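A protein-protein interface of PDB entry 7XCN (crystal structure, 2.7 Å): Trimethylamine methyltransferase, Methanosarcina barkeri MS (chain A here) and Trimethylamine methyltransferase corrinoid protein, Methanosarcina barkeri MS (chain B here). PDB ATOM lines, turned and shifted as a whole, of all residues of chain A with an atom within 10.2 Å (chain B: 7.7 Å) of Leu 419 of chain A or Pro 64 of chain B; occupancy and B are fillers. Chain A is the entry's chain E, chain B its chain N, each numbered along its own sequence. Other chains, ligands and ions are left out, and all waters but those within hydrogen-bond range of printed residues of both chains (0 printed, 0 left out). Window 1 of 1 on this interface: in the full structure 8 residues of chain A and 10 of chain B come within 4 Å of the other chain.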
ATOM      1  N   SER A 408      33.857 -15.922 -28.087  1.00  0.00           N
ATOM      2  CA  SER A 408      32.849 -14.887 -27.931  1.00  0.00           C
ATOM      3  C   SER A 408      33.540 -13.536 -27.902  1.00  0.00           C
ATOM      4  O   SER A 408      33.100 -12.584 -28.550  1.00  0.00           O
ATOM      5  CB  SER A 408      32.068 -15.081 -26.637  1.00  0.00           C
ATOM      6  OG  SER A 408      31.402 -16.324 -26.637  1.00  0.00           O
ATOM      7  N   VAL A 412      32.809 -10.729 -30.639  1.00  0.00           N
ATOM      8  CA  VAL A 412      32.328  -9.394 -30.303  1.00  0.00           C
ATOM      9  C   VAL A 412      33.352  -8.343 -30.717  1.00  0.00           C
ATOM     10  O   VAL A 412      33.002  -7.296 -31.259  1.00  0.00           O
ATOM     11  CB  VAL A 412      32.034  -9.258 -28.778  1.00  0.00           C
ATOM     12  CG1 VAL A 412      31.783  -7.798 -28.415  1.00  0.00           C
ATOM     13  CG2 VAL A 412      30.814 -10.104 -28.395  1.00  0.00           C
ATOM     14  N   ASN A 416      32.654  -3.321 -28.568  1.00  0.00           N
ATOM     15  CA  ASN A 416      31.265  -3.711 -28.778  1.00  0.00           C
ATOM     16  C   ASN A 416      30.750  -4.398 -27.534  1.00  0.00           C
ATOM     17  O   ASN A 416      31.504  -4.550 -26.573  1.00  0.00           O
ATOM     18  CB  ASN A 416      31.175  -4.632 -29.987  1.00  0.00           C
ATOM     19  CG  ASN A 416      31.682  -3.965 -31.239  1.00  0.00           C
ATOM     20  OD1 ASN A 416      32.424  -4.561 -32.016  1.00  0.00           O
ATOM     21  ND2 ASN A 416      31.283  -2.714 -31.442  1.00  0.00           N
ATOM     22  N   ASN A 417      29.478  -4.797 -27.531  1.00  0.00           N
ATOM     23  CA  ASN A 417      28.931  -5.469 -26.354  1.00  0.00           C
ATOM     24  C   ASN A 417      28.484  -6.897 -26.631  1.00  0.00           C
ATOM     25  O   ASN A 417      28.524  -7.360 -27.776  1.00  0.00           O
ATOM     26  CB  ASN A 417      27.793  -4.653 -25.743  1.00  0.00           C
ATOM     27  CG  ASN A 417      26.596  -4.551 -26.647  1.00  0.00           C
ATOM     28  OD1 ASN A 417      25.951  -5.550 -26.958  1.00  0.00           O
ATOM     29  ND2 ASN A 417      26.281  -3.333 -27.072  1.00  0.00           N
ATOM     30  N   PHE A 418      28.074  -7.594 -25.572  1.00  0.00           N
ATOM     31  CA  PHE A 418      27.662  -8.998 -25.658  1.00  0.00           C
ATOM     32  C   PHE A 418      26.167  -9.218 -25.489  1.00  0.00           C
ATOM     33  O   PHE A 418      25.708 -10.357 -25.477  1.00  0.00           O
ATOM     34  CB  PHE A 418      28.379  -9.829 -24.580  1.00  0.00           C
ATOM     35  CG  PHE A 418      29.871  -9.886 -24.728  1.00  0.00           C
ATOM     36  CD1 PHE A 418      30.645  -8.728 -24.656  1.00  0.00           C
ATOM     37  CD2 PHE A 418      30.508 -11.108 -24.924  1.00  0.00           C
ATOM     38  CE1 PHE A 418      32.025  -8.784 -24.776  1.00  0.00           C
ATOM     39  CE2 PHE A 418      31.893 -11.182 -25.046  1.00  0.00           C
ATOM     40  CZ  PHE A 418      32.655 -10.017 -24.972  1.00  0.00           C
ATOM     41  N   LEU A 419      25.414  -8.136 -25.352  1.00  0.00           N
ATOM     42  CA  LEU A 419      23.974  -8.220 -25.151  1.00  0.00           C
ATOM     43  C   LEU A 419      23.206  -9.090 -26.141  1.00  0.00           C
ATOM     44  O   LEU A 419      22.278  -9.795 -25.750  1.00  0.00           O
ATOM     45  CB  LEU A 419      23.372  -6.808 -25.136  1.00  0.00           C
ATOM     46  CG  LEU A 419      23.749  -5.920 -23.941  1.00  0.00           C
ATOM     47  CD1 LEU A 419      23.280  -4.497 -24.178  1.00  0.00           C
ATOM     48  CD2 LEU A 419      23.128  -6.482 -22.674  1.00  0.00           C
ATOM     49  N   ALA A 420      23.592  -9.066 -27.414  1.00  0.00           N
ATOM     50  CA  ALA A 420      22.869  -9.833 -28.427  1.00  0.00           C
ATOM     51  C   ALA A 420      23.412 -11.211 -28.787  1.00  0.00           C
ATOM     52  O   ALA A 420      22.890 -11.862 -29.684  1.00  0.00           O
ATOM     53  CB  ALA A 420      22.717  -9.000 -29.695  1.00  0.00           C
ATOM     54  N   LEU A 421      24.456 -11.665 -28.109  1.00  0.00           N
ATOM     55  CA  LEU A 421      25.002 -12.986 -28.408  1.00  0.00           C
ATOM     56  C   LEU A 421      24.041 -14.089 -27.984  1.00  0.00           C
ATOM     57  O   LEU A 421      23.261 -13.925 -27.043  1.00  0.00           O
ATOM     58  CB  LEU A 421      26.320 -13.213 -27.677  1.00  0.00           C
ATOM     59  CG  LEU A 421      27.556 -12.480 -28.161  1.00  0.00           C
ATOM     60  CD1 LEU A 421      28.727 -12.844 -27.262  1.00  0.00           C
ATOM     61  CD2 LEU A 421      27.841 -12.860 -29.599  1.00  0.00           C
ATOM     62  N   LYS A 422      24.106 -15.216 -28.682  1.00  0.00           N
ATOM     63  CA  LYS A 422      23.261 -16.355 -28.360  1.00  0.00           C
ATOM     64  C   LYS A 422      23.619 -16.771 -26.943  1.00  0.00           C
ATOM     65  O   LYS A 422      22.750 -17.033 -26.099  1.00  0.00           O
ATOM     66  CB  LYS A 422      23.543 -17.510 -29.330  1.00  0.00           C
ATOM     67  CG  LYS A 422      22.826 -18.816 -29.004  1.00  0.00           C
ATOM     68  CD  LYS A 422      23.097 -19.852 -30.077  1.00  0.00           C
ATOM     69  CE  LYS A 422      22.381 -21.162 -29.796  1.00  0.00           C
ATOM     70  NZ  LYS A 422      22.697 -22.204 -30.821  1.00  0.00           N
ATOM     71  N   GLN A 423      24.926 -16.811 -26.703  1.00  0.00           N
ATOM     72  CA  GLN A 423      25.502 -17.184 -25.419  1.00  0.00           C
ATOM     73  C   GLN A 423      24.832 -16.413 -24.279  1.00  0.00           C
ATOM     74  O   GLN A 423      24.317 -17.005 -23.334  1.00  0.00           O
ATOM     75  CB  GLN A 423      27.005 -16.900 -25.456  1.00  0.00           C
ATOM     76  CG  GLN A 423      27.801 -17.497 -24.316  1.00  0.00           C
ATOM     77  CD  GLN A 423      29.276 -17.120 -24.381  1.00  0.00           C
ATOM     78  OE1 GLN A 423      29.634 -15.938 -24.316  1.00  0.00           O
ATOM     79  NE2 GLN A 423      30.141 -18.127 -24.507  1.00  0.00           N
ATOM     80  N   THR A 424      24.828 -15.088 -24.384  1.00  0.00           N
ATOM     81  CA  THR A 424      24.221 -14.237 -23.369  1.00  0.00           C
ATOM     82  C   THR A 424      22.740 -14.525 -23.106  1.00  0.00           C
ATOM     83  O   THR A 424      22.318 -14.541 -21.958  1.00  0.00           O
ATOM     84  CB  THR A 424      24.342 -12.757 -23.746  1.00  0.00           C
ATOM     85  OG1 THR A 424      25.724 -12.420 -23.930  1.00  0.00           O
ATOM     86  CG2 THR A 424      23.725 -11.884 -22.654  1.00  0.00           C
ATOM     87  N   ARG A 425      21.951 -14.738 -24.159  1.00  0.00           N
ATOM     88  CA  ARG A 425      20.513 -14.999 -24.005  1.00  0.00           C
ATOM     89  C   ARG A 425      20.246 -16.318 -23.299  1.00  0.00           C
ATOM     90  O   ARG A 425      19.441 -16.397 -22.365  1.00  0.00           O
ATOM     91  CB  ARG A 425      19.813 -15.051 -25.360  1.00  0.00           C
ATOM     92  CG  ARG A 425      20.043 -13.857 -26.268  1.00  0.00           C
ATOM     93  CD  ARG A 425      19.155 -13.982 -27.499  1.00  0.00           C
ATOM     94  NE  ARG A 425      19.326 -15.258 -28.200  1.00  0.00           N
ATOM     95  CZ  ARG A 425      20.131 -15.447 -29.244  1.00  0.00           C
ATOM     96  NH1 ARG A 425      20.860 -14.441 -29.727  1.00  0.00           N
ATOM     97  NH2 ARG A 425      20.196 -16.641 -29.818  1.00  0.00           N
ATOM     98  N   GLN A 426      20.913 -17.363 -23.767  1.00  0.00           N
ATOM     99  CA  GLN A 426      20.733 -18.685 -23.193  1.00  0.00           C
ATOM    100  C   GLN A 426      21.028 -18.722 -21.700  1.00  0.00           C
ATOM    101  O   GLN A 426      20.490 -19.565 -20.980  1.00  0.00           O
ATOM    102  CB  GLN A 426      21.629 -19.688 -23.912  1.00  0.00           C
ATOM    103  CG  GLN A 426      21.388 -19.763 -25.398  1.00  0.00           C
ATOM    104  CD  GLN A 426      22.348 -20.710 -26.088  1.00  0.00           C
ATOM    105  OE1 GLN A 426      23.571 -20.545 -26.016  1.00  0.00           O
ATOM    106  NE2 GLN A 426      21.801 -21.709 -26.764  1.00  0.00           N
ATOM    107  N   LEU A 427      21.876 -17.808 -21.237  1.00  0.00           N
ATOM    108  CA  LEU A 427      22.256 -17.764 -19.828  1.00  0.00           C
ATOM    109  C   LEU A 427      21.612 -16.634 -19.034  1.00  0.00           C
ATOM    110  O   LEU A 427      22.058 -16.323 -17.923  1.00  0.00           O
ATOM    111  CB  LEU A 427      23.768 -17.622 -19.706  1.00  0.00           C
ATOM    112  CG  LEU A 427      24.641 -18.726 -20.284  1.00  0.00           C
ATOM    113  CD1 LEU A 427      26.094 -18.326 -20.123  1.00  0.00           C
ATOM    114  CD2 LEU A 427      24.361 -20.040 -19.583  1.00  0.00           C
ATOM    115  N   VAL A 428      20.567 -16.025 -19.588  1.00  0.00           N
ATOM    116  CA  VAL A 428      19.910 -14.910 -18.913  1.00  0.00           C
ATOM    117  C   VAL A 428      19.477 -15.224 -17.476  1.00  0.00           C
ATOM    118  O   VAL A 428      19.382 -14.320 -16.644  1.00  0.00           O
ATOM    119  CB  VAL A 428      18.687 -14.411 -19.717  1.00  0.00           C
ATOM    120  CG1 VAL A 428      17.575 -15.444 -19.669  1.00  0.00           C
ATOM    121  CG2 VAL A 428      18.220 -13.064 -19.169  1.00  0.00           C
ATOM    122  N   ASP A 429      19.224 -16.496 -17.184  1.00  0.00           N
ATOM    123  CA  ASP A 429      18.802 -16.891 -15.842  1.00  0.00           C
ATOM    124  C   ASP A 429      19.939 -17.295 -14.912  1.00  0.00           C
ATOM    125  O   ASP A 429      19.705 -17.554 -13.733  1.00  0.00           O
ATOM    126  CB  ASP A 429      17.808 -18.053 -15.890  1.00  0.00           C
ATOM    127  CG  ASP A 429      16.509 -17.692 -16.587  1.00  0.00           C
ATOM    128  OD1 ASP A 429      16.155 -16.493 -16.646  1.00  0.00           O
ATOM    129  OD2 ASP A 429      15.831 -18.627 -17.062  1.00  0.00           O
ATOM    130  N   TYR A 430      21.163 -17.350 -15.429  1.00  0.00           N
ATOM    131  CA  TYR A 430      22.308 -17.746 -14.617  1.00  0.00           C
ATOM    132  C   TYR A 430      22.729 -16.704 -13.569  1.00  0.00           C
ATOM    133  O   TYR A 430      22.859 -17.020 -12.387  1.00  0.00           O
ATOM    134  CB  TYR A 430      23.499 -18.093 -15.522  1.00  0.00           C
ATOM    135  CG  TYR A 430      24.663 -18.722 -14.784  1.00  0.00           C
ATOM    136  CD1 TYR A 430      24.460 -19.805 -13.920  1.00  0.00           C
ATOM    137  CD2 TYR A 430      25.965 -18.232 -14.934  1.00  0.00           C
ATOM    138  CE1 TYR A 430      25.522 -20.386 -13.220  1.00  0.00           C
ATOM    139  CE2 TYR A 430      27.039 -18.809 -14.238  1.00  0.00           C
ATOM    140  CZ  TYR A 430      26.806 -19.886 -13.381  1.00  0.00           C
ATOM    141  OH  TYR A 430      27.844 -20.460 -12.673  1.00  0.00           O
ATOM    142  N   PRO A 431      22.950 -15.447 -13.988  1.00  0.00           N
ATOM    143  CA  PRO A 431      23.359 -14.406 -13.038  1.00  0.00           C
ATOM    144  C   PRO A 431      22.426 -14.326 -11.832  1.00  0.00           C
ATOM    145  O   PRO A 431      21.253 -14.692 -11.930  1.00  0.00           O
ATOM    146  CB  PRO A 431      23.317 -13.135 -13.881  1.00  0.00           C
ATOM    147  CG  PRO A 431      23.658 -13.640 -15.248  1.00  0.00           C
ATOM    148  CD  PRO A 431      22.845 -14.902 -15.352  1.00  0.00           C
ATOM    149  N   PHE B  18      15.857 -15.837 -32.777  1.00  0.00           N
ATOM    150  CA  PHE B  18      17.111 -15.105 -32.740  1.00  0.00           C
ATOM    151  C   PHE B  18      18.101 -15.956 -33.509  1.00  0.00           C
ATOM    152  O   PHE B  18      19.025 -16.525 -32.928  1.00  0.00           O
ATOM    153  CB  PHE B  18      17.570 -14.968 -31.288  1.00  0.00           C
ATOM    154  CG  PHE B  18      16.438 -14.813 -30.313  1.00  0.00           C
ATOM    155  CD1 PHE B  18      15.858 -13.561 -30.089  1.00  0.00           C
ATOM    156  CD2 PHE B  18      15.915 -15.930 -29.656  1.00  0.00           C
ATOM    157  CE1 PHE B  18      14.776 -13.426 -29.226  1.00  0.00           C
ATOM    158  CE2 PHE B  18      14.826 -15.807 -28.788  1.00  0.00           C
ATOM    159  CZ  PHE B  18      14.255 -14.555 -28.572  1.00  0.00           C
ATOM    160  N   VAL B  52       8.280 -10.626 -29.861  1.00  0.00           N
ATOM    161  CA  VAL B  52       9.309 -10.609 -28.835  1.00  0.00           C
ATOM    162  C   VAL B  52       9.020  -9.440 -27.911  1.00  0.00           C
ATOM    163  O   VAL B  52       9.112  -9.556 -26.692  1.00  0.00           O
ATOM    164  CB  VAL B  52      10.712 -10.438 -29.455  1.00  0.00           C
ATOM    165  CG1 VAL B  52      11.757 -10.340 -28.362  1.00  0.00           C
ATOM    166  CG2 VAL B  52      11.020 -11.612 -30.372  1.00  0.00           C
ATOM    167  N   PHE B  56       8.518  -9.542 -23.937  1.00  0.00           N
ATOM    168  CA  PHE B  56       9.446  -8.735 -23.161  1.00  0.00           C
ATOM    169  C   PHE B  56       8.621  -7.879 -22.203  1.00  0.00           C
ATOM    170  O   PHE B  56       8.994  -7.679 -21.044  1.00  0.00           O
ATOM    171  CB  PHE B  56      10.254  -7.827 -24.084  1.00  0.00           C
ATOM    172  CG  PHE B  56      11.134  -6.858 -23.357  1.00  0.00           C
ATOM    173  CD1 PHE B  56      12.253  -7.303 -22.657  1.00  0.00           C
ATOM    174  CD2 PHE B  56      10.855  -5.495 -23.385  1.00  0.00           C
ATOM    175  CE1 PHE B  56      13.089  -6.396 -21.995  1.00  0.00           C
ATOM    176  CE2 PHE B  56      11.682  -4.581 -22.726  1.00  0.00           C
ATOM    177  CZ  PHE B  56      12.802  -5.031 -22.031  1.00  0.00           C
ATOM    178  N   LEU B  61      10.685 -12.317 -21.477  1.00  0.00           N
ATOM    179  CA  LEU B  61      11.961 -12.166 -22.171  1.00  0.00           C
ATOM    180  C   LEU B  61      12.608 -10.877 -21.678  1.00  0.00           C
ATOM    181  O   LEU B  61      11.926 -10.019 -21.112  1.00  0.00           O
ATOM    182  CB  LEU B  61      11.758 -12.079 -23.692  1.00  0.00           C
ATOM    183  CG  LEU B  61      11.025 -13.190 -24.455  1.00  0.00           C
ATOM    184  CD1 LEU B  61      11.087 -12.868 -25.950  1.00  0.00           C
ATOM    185  CD2 LEU B  61      11.643 -14.550 -24.175  1.00  0.00           C
ATOM    186  N   PHE B  62      13.917 -10.738 -21.894  1.00  0.00           N
ATOM    187  CA  PHE B  62      14.637  -9.542 -21.455  1.00  0.00           C
ATOM    188  C   PHE B  62      15.621  -9.048 -22.515  1.00  0.00           C
ATOM    189  O   PHE B  62      15.646  -9.558 -23.634  1.00  0.00           O
ATOM    190  CB  PHE B  62      15.388  -9.825 -20.147  1.00  0.00           C
ATOM    191  CG  PHE B  62      14.640 -10.722 -19.188  1.00  0.00           C
ATOM    192  CD1 PHE B  62      14.509 -12.090 -19.446  1.00  0.00           C
ATOM    193  CD2 PHE B  62      14.068 -10.201 -18.027  1.00  0.00           C
ATOM    194  CE1 PHE B  62      13.820 -12.923 -18.560  1.00  0.00           C
ATOM    195  CE2 PHE B  62      13.376 -11.026 -17.130  1.00  0.00           C
ATOM    196  CZ  PHE B  62      13.252 -12.387 -17.398  1.00  0.00           C
ATOM    197  N   LEU B  63      16.432  -8.059 -22.150  1.00  0.00           N
ATOM    198  CA  LEU B  63      17.426  -7.464 -23.052  1.00  0.00           C
ATOM    199  C   LEU B  63      18.155  -8.416 -24.013  1.00  0.00           C
ATOM    200  O   LEU B  63      18.184  -8.176 -25.215  1.00  0.00           O
ATOM    201  CB  LEU B  63      18.467  -6.678 -22.244  1.00  0.00           C
ATOM    202  CG  LEU B  63      17.929  -5.444 -21.523  1.00  0.00           C
ATOM    203  CD1 LEU B  63      19.034  -4.778 -20.717  1.00  0.00           C
ATOM    204  CD2 LEU B  63      17.355  -4.483 -22.553  1.00  0.00           C
ATOM    205  N   PRO B  64      18.765  -9.496 -23.498  1.00  0.00           N
ATOM    206  CA  PRO B  64      19.453 -10.389 -24.430  1.00  0.00           C
ATOM    207  C   PRO B  64      18.583 -10.679 -25.638  1.00  0.00           C
ATOM    208  O   PRO B  64      19.025 -10.529 -26.773  1.00  0.00           O
ATOM    209  CB  PRO B  64      19.711 -11.631 -23.589  1.00  0.00           C
ATOM    210  CG  PRO B  64      19.931 -11.056 -22.231  1.00  0.00           C
ATOM    211  CD  PRO B  64      18.824 -10.026 -22.123  1.00  0.00           C
ATOM    212  N   HIS B  65      17.339 -11.074 -25.383  1.00  0.00           N
ATOM    213  CA  HIS B  65      16.385 -11.387 -26.449  1.00  0.00           C
ATOM    214  C   HIS B  65      16.054 -10.207 -27.382  1.00  0.00           C
ATOM    215  O   HIS B  65      16.054 -10.348 -28.606  1.00  0.00           O
ATOM    216  CB  HIS B  65      15.099 -11.933 -25.834  1.00  0.00           C
ATOM    217  CG  HIS B  65      15.324 -13.095 -24.920  1.00  0.00           C
ATOM    218  ND1 HIS B  65      15.123 -13.020 -23.559  1.00  0.00           N
ATOM    219  CD2 HIS B  65      15.766 -14.350 -25.168  1.00  0.00           C
ATOM    220  CE1 HIS B  65      15.431 -14.181 -23.008  1.00  0.00           C
ATOM    221  NE2 HIS B  65      15.826 -15.006 -23.963  1.00  0.00           N
ATOM    222  N   VAL B  66      15.773  -9.048 -26.799  1.00  0.00           N
ATOM    223  CA  VAL B  66      15.446  -7.864 -27.574  1.00  0.00           C
ATOM    224  C   VAL B  66      16.530  -7.459 -28.566  1.00  0.00           C
ATOM    225  O   VAL B  66      16.225  -7.079 -29.694  1.00  0.00           O
ATOM    226  CB  VAL B  66      15.157  -6.674 -26.648  1.00  0.00           C
ATOM    227  CG1 VAL B  66      15.067  -5.377 -27.455  1.00  0.00           C
ATOM    228  CG2 VAL B  66      13.865  -6.923 -25.906  1.00  0.00           C
ATOM    229  N   LEU B  67      17.787  -7.524 -28.152  1.00  0.00           N
ATOM    230  CA  LEU B  67      18.879  -7.148 -29.037  1.00  0.00           C
ATOM    231  C   LEU B  67      19.192  -8.223 -30.040  1.00  0.00           C
ATOM    232  O   LEU B  67      19.632  -7.929 -31.150  1.00  0.00           O
ATOM    233  CB  LEU B  67      20.143  -6.822 -28.251  1.00  0.00           C
ATOM    234  CG  LEU B  67      20.138  -5.392 -27.714  1.00  0.00           C
ATOM    235  CD1 LEU B  67      19.320  -5.330 -26.433  1.00  0.00           C
ATOM    236  CD2 LEU B  67      21.570  -4.933 -27.484  1.00  0.00           C
ATOM    237  N   ALA B  68      18.975  -9.472 -29.650  1.00  0.00           N
ATOM    238  CA  ALA B  68      19.227 -10.595 -30.543  1.00  0.00           C
ATOM    239  C   ALA B  68      18.221 -10.533 -31.680  1.00  0.00           C
ATOM    240  O   ALA B  68      18.589 -10.648 -32.849  1.00  0.00           O
ATOM    241  CB  ALA B  68      19.092 -11.918 -29.794  1.00  0.00           C
ATOM    242  N   ALA B  69      16.951 -10.343 -31.330  1.00  0.00           N
ATOM    243  CA  ALA B  69      15.886 -10.262 -32.325  1.00  0.00           C
ATOM    244  C   ALA B  69      16.161  -9.135 -33.323  1.00  0.00           C
ATOM    245  O   ALA B  69      16.089  -9.338 -34.525  1.00  0.00           O
ATOM    246  CB  ALA B  69      14.557 -10.050 -31.637  1.00  0.00           C
ATOM    247  N   ALA B  70      16.490  -7.951 -32.827  1.00  0.00           N
ATOM    248  CA  ALA B  70      16.795  -6.826 -33.705  1.00  0.00           C
ATOM    249  C   ALA B  70      17.962  -7.164 -34.636  1.00  0.00           C
ATOM    250  O   ALA B  70      18.028  -6.679 -35.766  1.00  0.00           O
ATOM    251  CB  ALA B  70      17.132  -5.580 -32.872  1.00  0.00           C
ATOM    252  N   GLU B  71      18.879  -7.996 -34.152  1.00  0.00           N
ATOM    253  CA  GLU B  71      20.048  -8.397 -34.927  1.00  0.00           C
ATOM    254  C   GLU B  71      19.728  -9.506 -35.934  1.00  0.00           C
ATOM    255  O   GLU B  71      20.301  -9.543 -37.024  1.00  0.00           O
ATOM    256  CB  GLU B  71      21.169  -8.871 -34.004  1.00  0.00           C
ATOM    257  CG  GLU B  71      22.500  -8.969 -34.712  1.00  0.00           C
ATOM    258  CD  GLU B  71      23.398 -10.030 -34.131  1.00  0.00           C
ATOM    259  OE1 GLU B  71      22.993 -11.211 -34.139  1.00  0.00           O
ATOM    260  OE2 GLU B  71      24.509  -9.683 -33.676  1.00  0.00           O
ATOM    261  N   SER B 108      28.121   3.533 -23.395  1.00  0.00           N
ATOM    262  CA  SER B 108      27.252   3.235 -24.528  1.00  0.00           C
ATOM    263  C   SER B 108      26.319   2.035 -24.385  1.00  0.00           C
ATOM    264  O   SER B 108      25.353   1.912 -25.147  1.00  0.00           O
ATOM    265  CB  SER B 108      28.099   3.043 -25.776  1.00  0.00           C
ATOM    266  OG  SER B 108      28.897   1.886 -25.642  1.00  0.00           O
ATOM    267  N   ILE B 109      26.597   1.146 -23.434  1.00  0.00           N
ATOM    268  CA  ILE B 109      25.744  -0.027 -23.236  1.00  0.00           C
ATOM    269  C   ILE B 109      24.272   0.389 -23.196  1.00  0.00           C
ATOM    270  O   ILE B 109      23.425  -0.189 -23.876  1.00  0.00           O
ATOM    271  CB  ILE B 109      26.097  -0.770 -21.924  1.00  0.00           C
ATOM    272  CG1 ILE B 109      27.503  -1.369 -22.020  1.00  0.00           C
ATOM    273  CG2 ILE B 109      25.074  -1.867 -21.654  1.00  0.00           C
ATOM    274  CD1 ILE B 109      27.640  -2.449 -23.076  1.00  0.00           C
ATOM    275  N   GLY B 110      23.976   1.407 -22.398  1.00  0.00           N
ATOM    276  CA  GLY B 110      22.611   1.891 -22.296  1.00  0.00           C
ATOM    277  C   GLY B 110      22.081   2.484 -23.590  1.00  0.00           C
ATOM    278  O   GLY B 110      21.007   2.103 -24.059  1.00  0.00           O
ATOM    279  N   ASP B 112      22.822   1.877 -26.425  1.00  0.00           N
ATOM    280  CA  ASP B 112      22.578   0.737 -27.307  1.00  0.00           C
ATOM    281  C   ASP B 112      21.291   0.025 -26.930  1.00  0.00           C
ATOM    282  O   ASP B 112      20.621  -0.554 -27.783  1.00  0.00           O
ATOM    283  CB  ASP B 112      23.728  -0.263 -27.224  1.00  0.00           C
ATOM    284  CG  ASP B 112      24.826   0.033 -28.210  1.00  0.00           C
ATOM    285  OD1 ASP B 112      25.393   1.144 -28.156  1.00  0.00           O
ATOM    286  OD2 ASP B 112      25.117  -0.851 -29.044  1.00  0.00           O
ATOM    287  N   ILE B 113      20.952   0.060 -25.645  1.00  0.00           N
ATOM    288  CA  ILE B 113      19.737  -0.591 -25.171  1.00  0.00           C
ATOM    289  C   ILE B 113      18.503   0.258 -25.474  1.00  0.00           C
ATOM    290  O   ILE B 113      17.469  -0.265 -25.903  1.00  0.00           O
ATOM    291  CB  ILE B 113      19.824  -0.892 -23.660  1.00  0.00           C
ATOM    292  CG1 ILE B 113      20.980  -1.866 -23.414  1.00  0.00           C
ATOM    293  CG2 ILE B 113      18.503  -1.475 -23.160  1.00  0.00           C
ATOM    294  CD1 ILE B 113      21.142  -2.302 -21.990  1.00  0.00           C
ATOM    295  N   SER B 116      17.885  -0.123 -29.132  1.00  0.00           N
ATOM    296  CA  SER B 116      17.252  -1.390 -29.485  1.00  0.00           C
ATOM    297  C   SER B 116      15.838  -1.497 -28.943  1.00  0.00           C
ATOM    298  O   SER B 116      14.984  -2.131 -29.557  1.00  0.00           O
ATOM    299  CB  SER B 116      18.086  -2.562 -28.977  1.00  0.00           C
ATOM    300  OG  SER B 116      19.384  -2.513 -29.540  1.00  0.00           O
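Asn 417 of chain A touches Ile 109 of chain B.
Leu 419 of chain A touches Leu 67 of chain B.
CD1 of Leu 419 of chain A touches CG1 of Ile 113 of chain B, at 3.6 Å.
O of Leu 67 of chain B touches CB of Ala 420 of chain A, at 3.6 Å.
Ala 420 of chain A touches Ala 68 of chain B (CB to N, 3.8 Å).
CG2 of Thr 424 of chain A touches CG of Pro 64 of chain B (3.9 Å).
Arg 425 of chain A touches Pro 64 of chain B.
CA of His 65 of chain B touches CD of Arg 425 of chain A, at 3.9 Å.
Ala 68 of chain B touches Arg 425 of chain A (CB to NH1, 3.1 Å).
Phe 62 of chain B touches Val 428 of chain A (CD1 to CG2, 3.8 Å).
The backbone carbonyl oxygen (O) of Ala 420 of chain A is in hydrogen-bond range of the guanidinium group (NH1) of Arg 425 of chain A (3.3 Å).
The backbone carbonyl oxygen (O) of Phe 418 of chain A lies within hydrogen-bond range of the side-chain hydroxyl (OG1) of Thr 424 of chain A.
The backbone NH of Phe 62 of chain B is in hydrogen-bond range of a ring nitrogen (ND1) of His 65 of chain B, at 3.1 Å.
OD1 of Asn 417 of chain A sits at hydrogen-bond distance from N of Leu 419 of chain A, at 3.1 Å.
The side-chain hydroxyl (OG) of Ser 116 of chain B lies within hydrogen-bond range of the backbone carbonyl oxygen (O) of Asp 112 of chain B, at 2.9 Å.
O of Pro 64 of chain B lies close to O of Leu 419 of chain A (3.5 Å).
The backbone carbonyl oxygen of Phe 18 of chain B lies within hydrogen-bond range of the guanidinium group of Arg 425 of chain A (3.3 Å).
ND2 of Asn 417 of chain A lies within hydrogen-bond range of OD2 of Asp 112 of chain B.
Leu 427 of chain A touches none of the printed residues of chain B.
Of the printed residues of chain B, Val 428 of chain A touches Phe 62.
Val 52 of chain B touches none of the printed residues of chain A.
Of the printed residues of chain A, Phe 62 of chain B touches Val 428 (3.8 Å).
No residue of chain A comes within 4 Å of Leu 63 of chain B.
Of the printed residues of chain A, Pro 64 of chain B touches Leu 419 (3.2 Å), Thr 424 (3.9 Å) and Arg 425 (3.5 Å).
His 65 of chain B touches just one residue of chain A: Arg 425.
Of chain A, only Leu 419 (3.5 Å) and Ala 420 (3.6 Å) come within 4 Å of Leu 67 of chain B.
Of chain A, only Ala 420 and Arg 425 come within 4 Å of Ala 68 of chain B.
The nearest printed residue of chain A that does not touch Ile 109 of chain B is Leu 419 of chain A (4.1 Å).
Of the 20 printed residues of chain B, 9 touch a printed residue of chain A.
Printed residues of chain B that touch a printed residue of chain A: Phe 18, Phe 62, Pro 64, His 65, Leu 67, Ala 68, Ile 109, Asp 112 and Ile 113.
Hydrophobic or aromatic side chains of chain B that line the printed part of chain A: Phe 18, Phe 62, Pro 64, Leu 67, Ala 68, Ile 109 and Ile 113.
Printed residues of chain A that touch a printed residue of chain B: Asn 417, Leu 419, Ala 420, Thr 424, Arg 425 and Val 428.
Hydrophobic or aromatic side chains of chain A that line the printed part of chain B: Leu 419, Ala 420 and Val 428.
Among the printed residues, 13 pairs touch across the chains.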
